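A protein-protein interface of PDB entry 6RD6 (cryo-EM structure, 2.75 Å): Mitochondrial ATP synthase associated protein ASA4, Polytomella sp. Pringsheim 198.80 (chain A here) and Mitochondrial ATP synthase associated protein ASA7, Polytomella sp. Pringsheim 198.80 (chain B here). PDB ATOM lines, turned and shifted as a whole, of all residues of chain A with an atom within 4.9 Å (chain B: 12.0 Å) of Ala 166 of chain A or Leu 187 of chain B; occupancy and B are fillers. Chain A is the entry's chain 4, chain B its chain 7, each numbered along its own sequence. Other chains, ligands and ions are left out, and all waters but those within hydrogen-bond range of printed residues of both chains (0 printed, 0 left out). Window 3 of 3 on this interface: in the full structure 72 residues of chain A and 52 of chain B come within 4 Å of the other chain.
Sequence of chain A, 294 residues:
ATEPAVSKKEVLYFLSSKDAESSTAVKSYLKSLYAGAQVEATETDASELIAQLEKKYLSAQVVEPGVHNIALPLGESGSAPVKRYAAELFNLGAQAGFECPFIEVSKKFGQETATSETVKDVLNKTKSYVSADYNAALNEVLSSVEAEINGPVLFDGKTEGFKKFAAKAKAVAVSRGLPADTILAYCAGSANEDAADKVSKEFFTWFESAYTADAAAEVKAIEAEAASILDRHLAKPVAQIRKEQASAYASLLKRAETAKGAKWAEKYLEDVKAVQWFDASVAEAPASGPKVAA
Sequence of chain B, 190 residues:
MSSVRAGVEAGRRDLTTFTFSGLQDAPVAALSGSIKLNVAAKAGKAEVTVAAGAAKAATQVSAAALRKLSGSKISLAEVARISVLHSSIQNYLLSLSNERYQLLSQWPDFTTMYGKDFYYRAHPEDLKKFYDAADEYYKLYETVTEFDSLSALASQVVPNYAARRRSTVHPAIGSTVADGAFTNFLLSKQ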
ATOM      1  N   PHE A 162      -9.514 -12.958  -8.471  1.00  0.00           N
ATOM      2  CA  PHE A 162     -10.318 -12.486  -7.354  1.00  0.00           C
ATOM      3  C   PHE A 162      -9.799 -11.162  -6.817  1.00  0.00           C
ATOM      4  O   PHE A 162     -10.572 -10.365  -6.287  1.00  0.00           O
ATOM      5  CB  PHE A 162     -10.374 -13.520  -6.231  1.00  0.00           C
ATOM      6  CG  PHE A 162     -11.373 -13.176  -5.161  1.00  0.00           C
ATOM      7  CD1 PHE A 162     -12.720 -13.425  -5.355  1.00  0.00           C
ATOM      8  CD2 PHE A 162     -10.973 -12.570  -3.978  1.00  0.00           C
ATOM      9  CE1 PHE A 162     -13.645 -13.095  -4.389  1.00  0.00           C
ATOM     10  CE2 PHE A 162     -11.895 -12.239  -3.008  1.00  0.00           C
ATOM     11  CZ  PHE A 162     -13.232 -12.506  -3.214  1.00  0.00           C
ATOM     12  N   LYS A 163      -8.499 -10.896  -6.956  1.00  0.00           N
ATOM     13  CA  LYS A 163      -7.976  -9.607  -6.514  1.00  0.00           C
ATOM     14  C   LYS A 163      -8.447  -8.479  -7.427  1.00  0.00           C
ATOM     15  O   LYS A 163      -8.781  -7.387  -6.953  1.00  0.00           O
ATOM     16  CB  LYS A 163      -6.453  -9.651  -6.441  1.00  0.00           C
ATOM     17  CG  LYS A 163      -5.930 -10.425  -5.248  1.00  0.00           C
ATOM     18  CD  LYS A 163      -4.637  -9.832  -4.726  1.00  0.00           C
ATOM     19  CE  LYS A 163      -4.169 -10.556  -3.476  1.00  0.00           C
ATOM     20  NZ  LYS A 163      -3.925 -12.003  -3.731  1.00  0.00           N
ATOM     21  N   LYS A 164      -8.520  -8.741  -8.735  1.00  0.00           N
ATOM     22  CA  LYS A 164      -9.059  -7.745  -9.657  1.00  0.00           C
ATOM     23  C   LYS A 164     -10.556  -7.546  -9.445  1.00  0.00           C
ATOM     24  O   LYS A 164     -11.053  -6.406  -9.473  1.00  0.00           O
ATOM     25  CB  LYS A 164      -8.764  -8.156 -11.099  1.00  0.00           C
ATOM     26  CG  LYS A 164      -7.328  -7.894 -11.526  1.00  0.00           C
ATOM     27  CD  LYS A 164      -7.104  -8.229 -12.989  1.00  0.00           C
ATOM     28  CE  LYS A 164      -6.971  -9.726 -13.196  1.00  0.00           C
ATOM     29  NZ  LYS A 164      -6.442 -10.048 -14.548  1.00  0.00           N
ATOM     30  N   PHE A 165     -11.287  -8.645  -9.206  1.00  0.00           N
ATOM     31  CA  PHE A 165     -12.705  -8.542  -8.873  1.00  0.00           C
ATOM     32  C   PHE A 165     -12.919  -7.793  -7.564  1.00  0.00           C
ATOM     33  O   PHE A 165     -13.867  -7.017  -7.444  1.00  0.00           O
ATOM     34  CB  PHE A 165     -13.344  -9.928  -8.787  1.00  0.00           C
ATOM     35  CG  PHE A 165     -14.714  -9.916  -8.167  1.00  0.00           C
ATOM     36  CD1 PHE A 165     -15.790  -9.402  -8.865  1.00  0.00           C
ATOM     37  CD2 PHE A 165     -14.922 -10.394  -6.879  1.00  0.00           C
ATOM     38  CE1 PHE A 165     -17.050  -9.369  -8.302  1.00  0.00           C
ATOM     39  CE2 PHE A 165     -16.177 -10.359  -6.310  1.00  0.00           C
ATOM     40  CZ  PHE A 165     -17.244  -9.848  -7.025  1.00  0.00           C
ATOM     41  N   ALA A 166     -12.040  -7.995  -6.583  1.00  0.00           N
ATOM     42  CA  ALA A 166     -12.197  -7.336  -5.294  1.00  0.00           C
ATOM     43  C   ALA A 166     -11.867  -5.857  -5.391  1.00  0.00           C
ATOM     44  O   ALA A 166     -12.484  -5.038  -4.704  1.00  0.00           O
ATOM     45  CB  ALA A 166     -11.319  -8.014  -4.246  1.00  0.00           C
ATOM     46  N   ALA A 167     -10.919  -5.493  -6.257  1.00  0.00           N
ATOM     47  CA  ALA A 167     -10.628  -4.079  -6.477  1.00  0.00           C
ATOM     48  C   ALA A 167     -11.798  -3.372  -7.152  1.00  0.00           C
ATOM     49  O   ALA A 167     -12.218  -2.290  -6.717  1.00  0.00           O
ATOM     50  CB  ALA A 167      -9.355  -3.927  -7.307  1.00  0.00           C
ATOM     51  N   LYS A 168     -12.367  -3.986  -8.195  1.00  0.00           N
ATOM     52  CA  LYS A 168     -13.507  -3.361  -8.864  1.00  0.00           C
ATOM     53  C   LYS A 168     -14.765  -3.403  -7.993  1.00  0.00           C
ATOM     54  O   LYS A 168     -15.610  -2.500  -8.064  1.00  0.00           O
ATOM     55  CB  LYS A 168     -13.750  -4.031 -10.212  1.00  0.00           C
ATOM     56  CG  LYS A 168     -12.704  -3.709 -11.262  1.00  0.00           C
ATOM     57  CD  LYS A 168     -12.877  -4.579 -12.495  1.00  0.00           C
ATOM     58  CE  LYS A 168     -14.141  -4.223 -13.253  1.00  0.00           C
ATOM     59  NZ  LYS A 168     -14.040  -2.873 -13.869  1.00  0.00           N
ATOM     60  N   ALA A 169     -14.884  -4.419  -7.133  1.00  0.00           N
ATOM     61  CA  ALA A 169     -16.016  -4.496  -6.220  1.00  0.00           C
ATOM     62  C   ALA A 169     -15.898  -3.467  -5.108  1.00  0.00           C
ATOM     63  O   ALA A 169     -16.904  -2.908  -4.663  1.00  0.00           O
ATOM     64  CB  ALA A 169     -16.126  -5.904  -5.639  1.00  0.00           C
ATOM     65  N   LYS A 170     -14.673  -3.190  -4.656  1.00  0.00           N
ATOM     66  CA  LYS A 170     -14.466  -2.097  -3.717  1.00  0.00           C
ATOM     67  C   LYS A 170     -14.769  -0.759  -4.372  1.00  0.00           C
ATOM     68  O   LYS A 170     -15.306   0.146  -3.724  1.00  0.00           O
ATOM     69  CB  LYS A 170     -13.036  -2.126  -3.188  1.00  0.00           C
ATOM     70  CG  LYS A 170     -12.795  -1.226  -1.997  1.00  0.00           C
ATOM     71  CD  LYS A 170     -11.373  -1.369  -1.501  1.00  0.00           C
ATOM     72  CE  LYS A 170     -11.147  -2.741  -0.895  1.00  0.00           C
ATOM     73  NZ  LYS A 170      -9.788  -2.882  -0.316  1.00  0.00           N
ATOM     74  N   ALA A 180     -16.079   0.963   2.097  1.00  0.00           N
ATOM     75  CA  ALA A 180     -15.672  -0.434   2.204  1.00  0.00           C
ATOM     76  C   ALA A 180     -14.340  -0.589   2.924  1.00  0.00           C
ATOM     77  O   ALA A 180     -14.087  -1.624   3.548  1.00  0.00           O
ATOM     78  CB  ALA A 180     -15.604  -1.061   0.813  1.00  0.00           C
ATOM     79  N   LEU A 184     -14.151  -2.875   6.172  1.00  0.00           N
ATOM     80  CA  LEU A 184     -13.158  -3.943   6.208  1.00  0.00           C
ATOM     81  C   LEU A 184     -12.206  -3.780   7.386  1.00  0.00           C
ATOM     82  O   LEU A 184     -11.838  -4.768   8.032  1.00  0.00           O
ATOM     83  CB  LEU A 184     -12.380  -3.977   4.898  1.00  0.00           C
ATOM     84  CG  LEU A 184     -13.019  -4.747   3.748  1.00  0.00           C
ATOM     85  CD1 LEU A 184     -12.412  -4.290   2.441  1.00  0.00           C
ATOM     86  CD2 LEU A 184     -12.833  -6.234   3.939  1.00  0.00           C
ATOM     87  N   ALA B 178     -27.080  -4.893   5.278  1.00  0.00           N
ATOM     88  CA  ALA B 178     -26.748  -6.153   4.625  1.00  0.00           C
ATOM     89  C   ALA B 178     -25.819  -5.933   3.440  1.00  0.00           C
ATOM     90  O   ALA B 178     -24.976  -6.783   3.144  1.00  0.00           O
ATOM     91  CB  ALA B 178     -28.025  -6.862   4.187  1.00  0.00           C
ATOM     92  N   ASP B 179     -25.922  -4.776   2.782  1.00  0.00           N
ATOM     93  CA  ASP B 179     -25.005  -4.454   1.692  1.00  0.00           C
ATOM     94  C   ASP B 179     -23.594  -4.208   2.206  1.00  0.00           C
ATOM     95  O   ASP B 179     -22.623  -4.685   1.612  1.00  0.00           O
ATOM     96  CB  ASP B 179     -25.508  -3.237   0.921  1.00  0.00           C
ATOM     97  CG  ASP B 179     -26.574  -3.587  -0.087  1.00  0.00           C
ATOM     98  OD1 ASP B 179     -27.029  -4.748  -0.097  1.00  0.00           O
ATOM     99  OD2 ASP B 179     -26.970  -2.696  -0.865  1.00  0.00           O
ATOM    100  N   GLY B 180     -23.460  -3.473   3.312  1.00  0.00           N
ATOM    101  CA  GLY B 180     -22.141  -3.258   3.892  1.00  0.00           C
ATOM    102  C   GLY B 180     -21.536  -4.529   4.457  1.00  0.00           C
ATOM    103  O   GLY B 180     -20.326  -4.760   4.349  1.00  0.00           O
ATOM    104  N   ALA B 181     -22.374  -5.393   5.028  1.00  0.00           N
ATOM    105  CA  ALA B 181     -21.881  -6.678   5.498  1.00  0.00           C
ATOM    106  C   ALA B 181     -21.516  -7.588   4.336  1.00  0.00           C
ATOM    107  O   ALA B 181     -20.627  -8.433   4.460  1.00  0.00           O
ATOM    108  CB  ALA B 181     -22.918  -7.340   6.390  1.00  0.00           C
ATOM    109  N   PHE B 182     -22.165  -7.413   3.185  1.00  0.00           N
ATOM    110  CA  PHE B 182     -21.772  -8.184   2.013  1.00  0.00           C
ATOM    111  C   PHE B 182     -20.475  -7.664   1.413  1.00  0.00           C
ATOM    112  O   PHE B 182     -19.705  -8.439   0.841  1.00  0.00           O
ATOM    113  CB  PHE B 182     -22.879  -8.176   0.969  1.00  0.00           C
ATOM    114  CG  PHE B 182     -22.734  -9.250  -0.058  1.00  0.00           C
ATOM    115  CD1 PHE B 182     -22.775 -10.582   0.310  1.00  0.00           C
ATOM    116  CD2 PHE B 182     -22.550  -8.932  -1.390  1.00  0.00           C
ATOM    117  CE1 PHE B 182     -22.643 -11.577  -0.633  1.00  0.00           C
ATOM    118  CE2 PHE B 182     -22.418  -9.922  -2.338  1.00  0.00           C
ATOM    119  CZ  PHE B 182     -22.464 -11.247  -1.959  1.00  0.00           C
ATOM    120  N   THR B 183     -20.217  -6.356   1.527  1.00  0.00           N
ATOM    121  CA  THR B 183     -18.897  -5.842   1.162  1.00  0.00           C
ATOM    122  C   THR B 183     -17.820  -6.437   2.054  1.00  0.00           C
ATOM    123  O   THR B 183     -16.758  -6.843   1.568  1.00  0.00           O
ATOM    124  CB  THR B 183     -18.831  -4.318   1.257  1.00  0.00           C
ATOM    125  OG1 THR B 183     -19.082  -3.908   2.605  1.00  0.00           O
ATOM    126  CG2 THR B 183     -19.820  -3.672   0.352  1.00  0.00           C
ATOM    127  N   ASN B 184     -18.086  -6.512   3.360  1.00  0.00           N
ATOM    128  CA  ASN B 184     -17.116  -7.112   4.272  1.00  0.00           C
ATOM    129  C   ASN B 184     -16.943  -8.605   4.011  1.00  0.00           C
ATOM    130  O   ASN B 184     -15.837  -9.139   4.139  1.00  0.00           O
ATOM    131  CB  ASN B 184     -17.532  -6.877   5.718  1.00  0.00           C
ATOM    132  CG  ASN B 184     -16.563  -7.482   6.698  1.00  0.00           C
ATOM    133  OD1 ASN B 184     -16.908  -8.389   7.451  1.00  0.00           O
ATOM    134  ND2 ASN B 184     -15.333  -6.997   6.680  1.00  0.00           N
ATOM    135  N   PHE B 185     -18.019  -9.287   3.620  1.00  0.00           N
ATOM    136  CA  PHE B 185     -17.947 -10.722   3.372  1.00  0.00           C
ATOM    137  C   PHE B 185     -17.223 -11.023   2.067  1.00  0.00           C
ATOM    138  O   PHE B 185     -16.437 -11.973   1.986  1.00  0.00           O
ATOM    139  CB  PHE B 185     -19.358 -11.305   3.357  1.00  0.00           C
ATOM    140  CG  PHE B 185     -19.426 -12.713   2.866  1.00  0.00           C
ATOM    141  CD1 PHE B 185     -19.984 -13.004   1.633  1.00  0.00           C
ATOM    142  CD2 PHE B 185     -18.942 -13.750   3.642  1.00  0.00           C
ATOM    143  CE1 PHE B 185     -20.049 -14.298   1.181  1.00  0.00           C
ATOM    144  CE2 PHE B 185     -19.007 -15.049   3.196  1.00  0.00           C
ATOM    145  CZ  PHE B 185     -19.559 -15.323   1.963  1.00  0.00           C
ATOM    146  N   LEU B 186     -17.469 -10.219   1.034  1.00  0.00           N
ATOM    147  CA  LEU B 186     -16.922 -10.504  -0.284  1.00  0.00           C
ATOM    148  C   LEU B 186     -15.480 -10.035  -0.399  1.00  0.00           C
ATOM    149  O   LEU B 186     -14.634 -10.735  -0.960  1.00  0.00           O
ATOM    150  CB  LEU B 186     -17.788  -9.841  -1.350  1.00  0.00           C
ATOM    151  CG  LEU B 186     -17.802 -10.459  -2.739  1.00  0.00           C
ATOM    152  CD1 LEU B 186     -18.348 -11.869  -2.679  1.00  0.00           C
ATOM    153  CD2 LEU B 186     -18.643  -9.596  -3.648  1.00  0.00           C
ATOM    154  N   LEU B 187     -15.174  -8.849   0.131  1.00  0.00           N
ATOM    155  CA  LEU B 187     -13.833  -8.302  -0.037  1.00  0.00           C
ATOM    156  C   LEU B 187     -12.838  -8.956   0.914  1.00  0.00           C
ATOM    157  O   LEU B 187     -11.623  -8.777   0.770  1.00  0.00           O
ATOM    158  CB  LEU B 187     -13.862  -6.789   0.148  1.00  0.00           C
ATOM    159  CG  LEU B 187     -14.712  -6.023  -0.869  1.00  0.00           C
ATOM    160  CD1 LEU B 187     -14.488  -4.532  -0.734  1.00  0.00           C
ATOM    161  CD2 LEU B 187     -14.443  -6.487  -2.289  1.00  0.00           C
ATOM    162  N   SER B 188     -13.327  -9.701   1.900  1.00  0.00           N
ATOM    163  CA  SER B 188     -12.464 -10.606   2.642  1.00  0.00           C
ATOM    164  C   SER B 188     -12.401 -11.952   1.928  1.00  0.00           C
ATOM    165  O   SER B 188     -13.254 -12.278   1.099  1.00  0.00           O
ATOM    166  CB  SER B 188     -12.973 -10.786   4.068  1.00  0.00           C
ATOM    167  OG  SER B 188     -12.954  -9.557   4.768  1.00  0.00           O
ATOM    168  N   LYS B 189     -11.376 -12.736   2.248  1.00  0.00           N
ATOM    169  CA  LYS B 189     -11.197 -14.009   1.566  1.00  0.00           C
ATOM    170  C   LYS B 189     -12.188 -15.048   2.086  1.00  0.00           C
ATOM    171  O   LYS B 189     -12.400 -15.176   3.297  1.00  0.00           O
ATOM    172  CB  LYS B 189      -9.750 -14.495   1.723  1.00  0.00           C
ATOM    173  CG  LYS B 189      -9.241 -14.609   3.155  1.00  0.00           C
ATOM    174  CD  LYS B 189      -7.732 -14.729   3.205  1.00  0.00           C
ATOM    175  CE  LYS B 189      -7.078 -13.382   2.984  1.00  0.00           C
ATOM    176  NZ  LYS B 189      -7.425 -12.429   4.071  1.00  0.00           N
ATOM    177  N   GLN B 190     -12.800 -15.774   1.144  1.00  0.00           N
ATOM    178  CA  GLN B 190     -13.799 -16.833   1.380  1.00  0.00           C
ATOM    179  C   GLN B 190     -14.960 -16.362   2.274  1.00  0.00           C
ATOM    180  O   GLN B 190     -16.023 -16.980   2.345  1.00  0.00           O
ATOM    181  CB  GLN B 190     -13.128 -18.078   1.981  1.00  0.00           C
ATOM    182  CG  GLN B 190     -13.931 -19.370   1.826  1.00  0.00           C
ATOM    183  CD  GLN B 190     -13.591 -20.410   2.875  1.00  0.00           C
ATOM    184  OE1 GLN B 190     -12.601 -21.129   2.755  1.00  0.00           O
ATOM    185  NE2 GLN B 190     -14.415 -20.495   3.913  1.00  0.00           N
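Phe 162 of chain A touches Leu 186 of chain B. Leu 186 of chain B touches Phe 165 of chain A (CD2 to CZ, 3.7 Å). Ala 166 of chain A touches Leu 187 of chain B (O to CD2, 3.4 Å). CB of Ala 169 of chain A touches CD2 of Leu 187 of chain B, 3.8 Å away. Lys 170 of chain A touches Leu 187 of chain B. Leu 187 of chain B touches Ala 180 of chain A. Leu 184 of chain A touches Asn 184 of chain B (CA to ND2, 3.8 Å). Leu 184 of chain A touches Leu 187 of chain B. Leu 184 of chain A touches Ser 188 of chain B.
The side-chain hydroxyl (OG) of Ser 188 of chain B sits at hydrogen-bond distance from the backbone carbonyl oxygen (O) of Asn 184 of chain B.
Printed residues of chain A that touch a printed residue of chain B: Phe 162, Phe 165, Ala 166, Ala 169, Lys 170, Ala 180 and Leu 184. Hydrophobic or aromatic side chains of chain A that line the printed part of chain B: Phe 162, Phe 165, Ala 166, Ala 169, Ala 180 and Leu 184. Of the 13 printed residues of chain B, 4 touch a printed residue of chain A. Among the printed residues, 9 pairs touch across the chains.
Ala 166 of chain A touches one residue of chain B. Of the printed residues of chain A, Leu 187 of chain B touches Ala 166, Ala 169, Lys 170, Ala 180 and Leu 184. Of the printed residues of chain B, Phe 165 of chain A touches Leu 186. No residue of chain B comes within 4 Å of Ala 167 of chain A. Ala 169 of chain A touches one residue of chain B. Ala 180 of chain A touches one residue of chain B. Of the printed residues of chain B, Leu 184 of chain A touches Asn 184, Leu 187 and Ser 188. Printed residues of chain A within 4 Å of Asn 184 of chain B: Leu 184. Of the printed residues of chain A, Ser 188 of chain B touches Leu 184 (3.4 Å). The nearest printed residue of chain A that does not touch Leu 187 of chain B is Phe 162 of chain A (5.1 Å).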
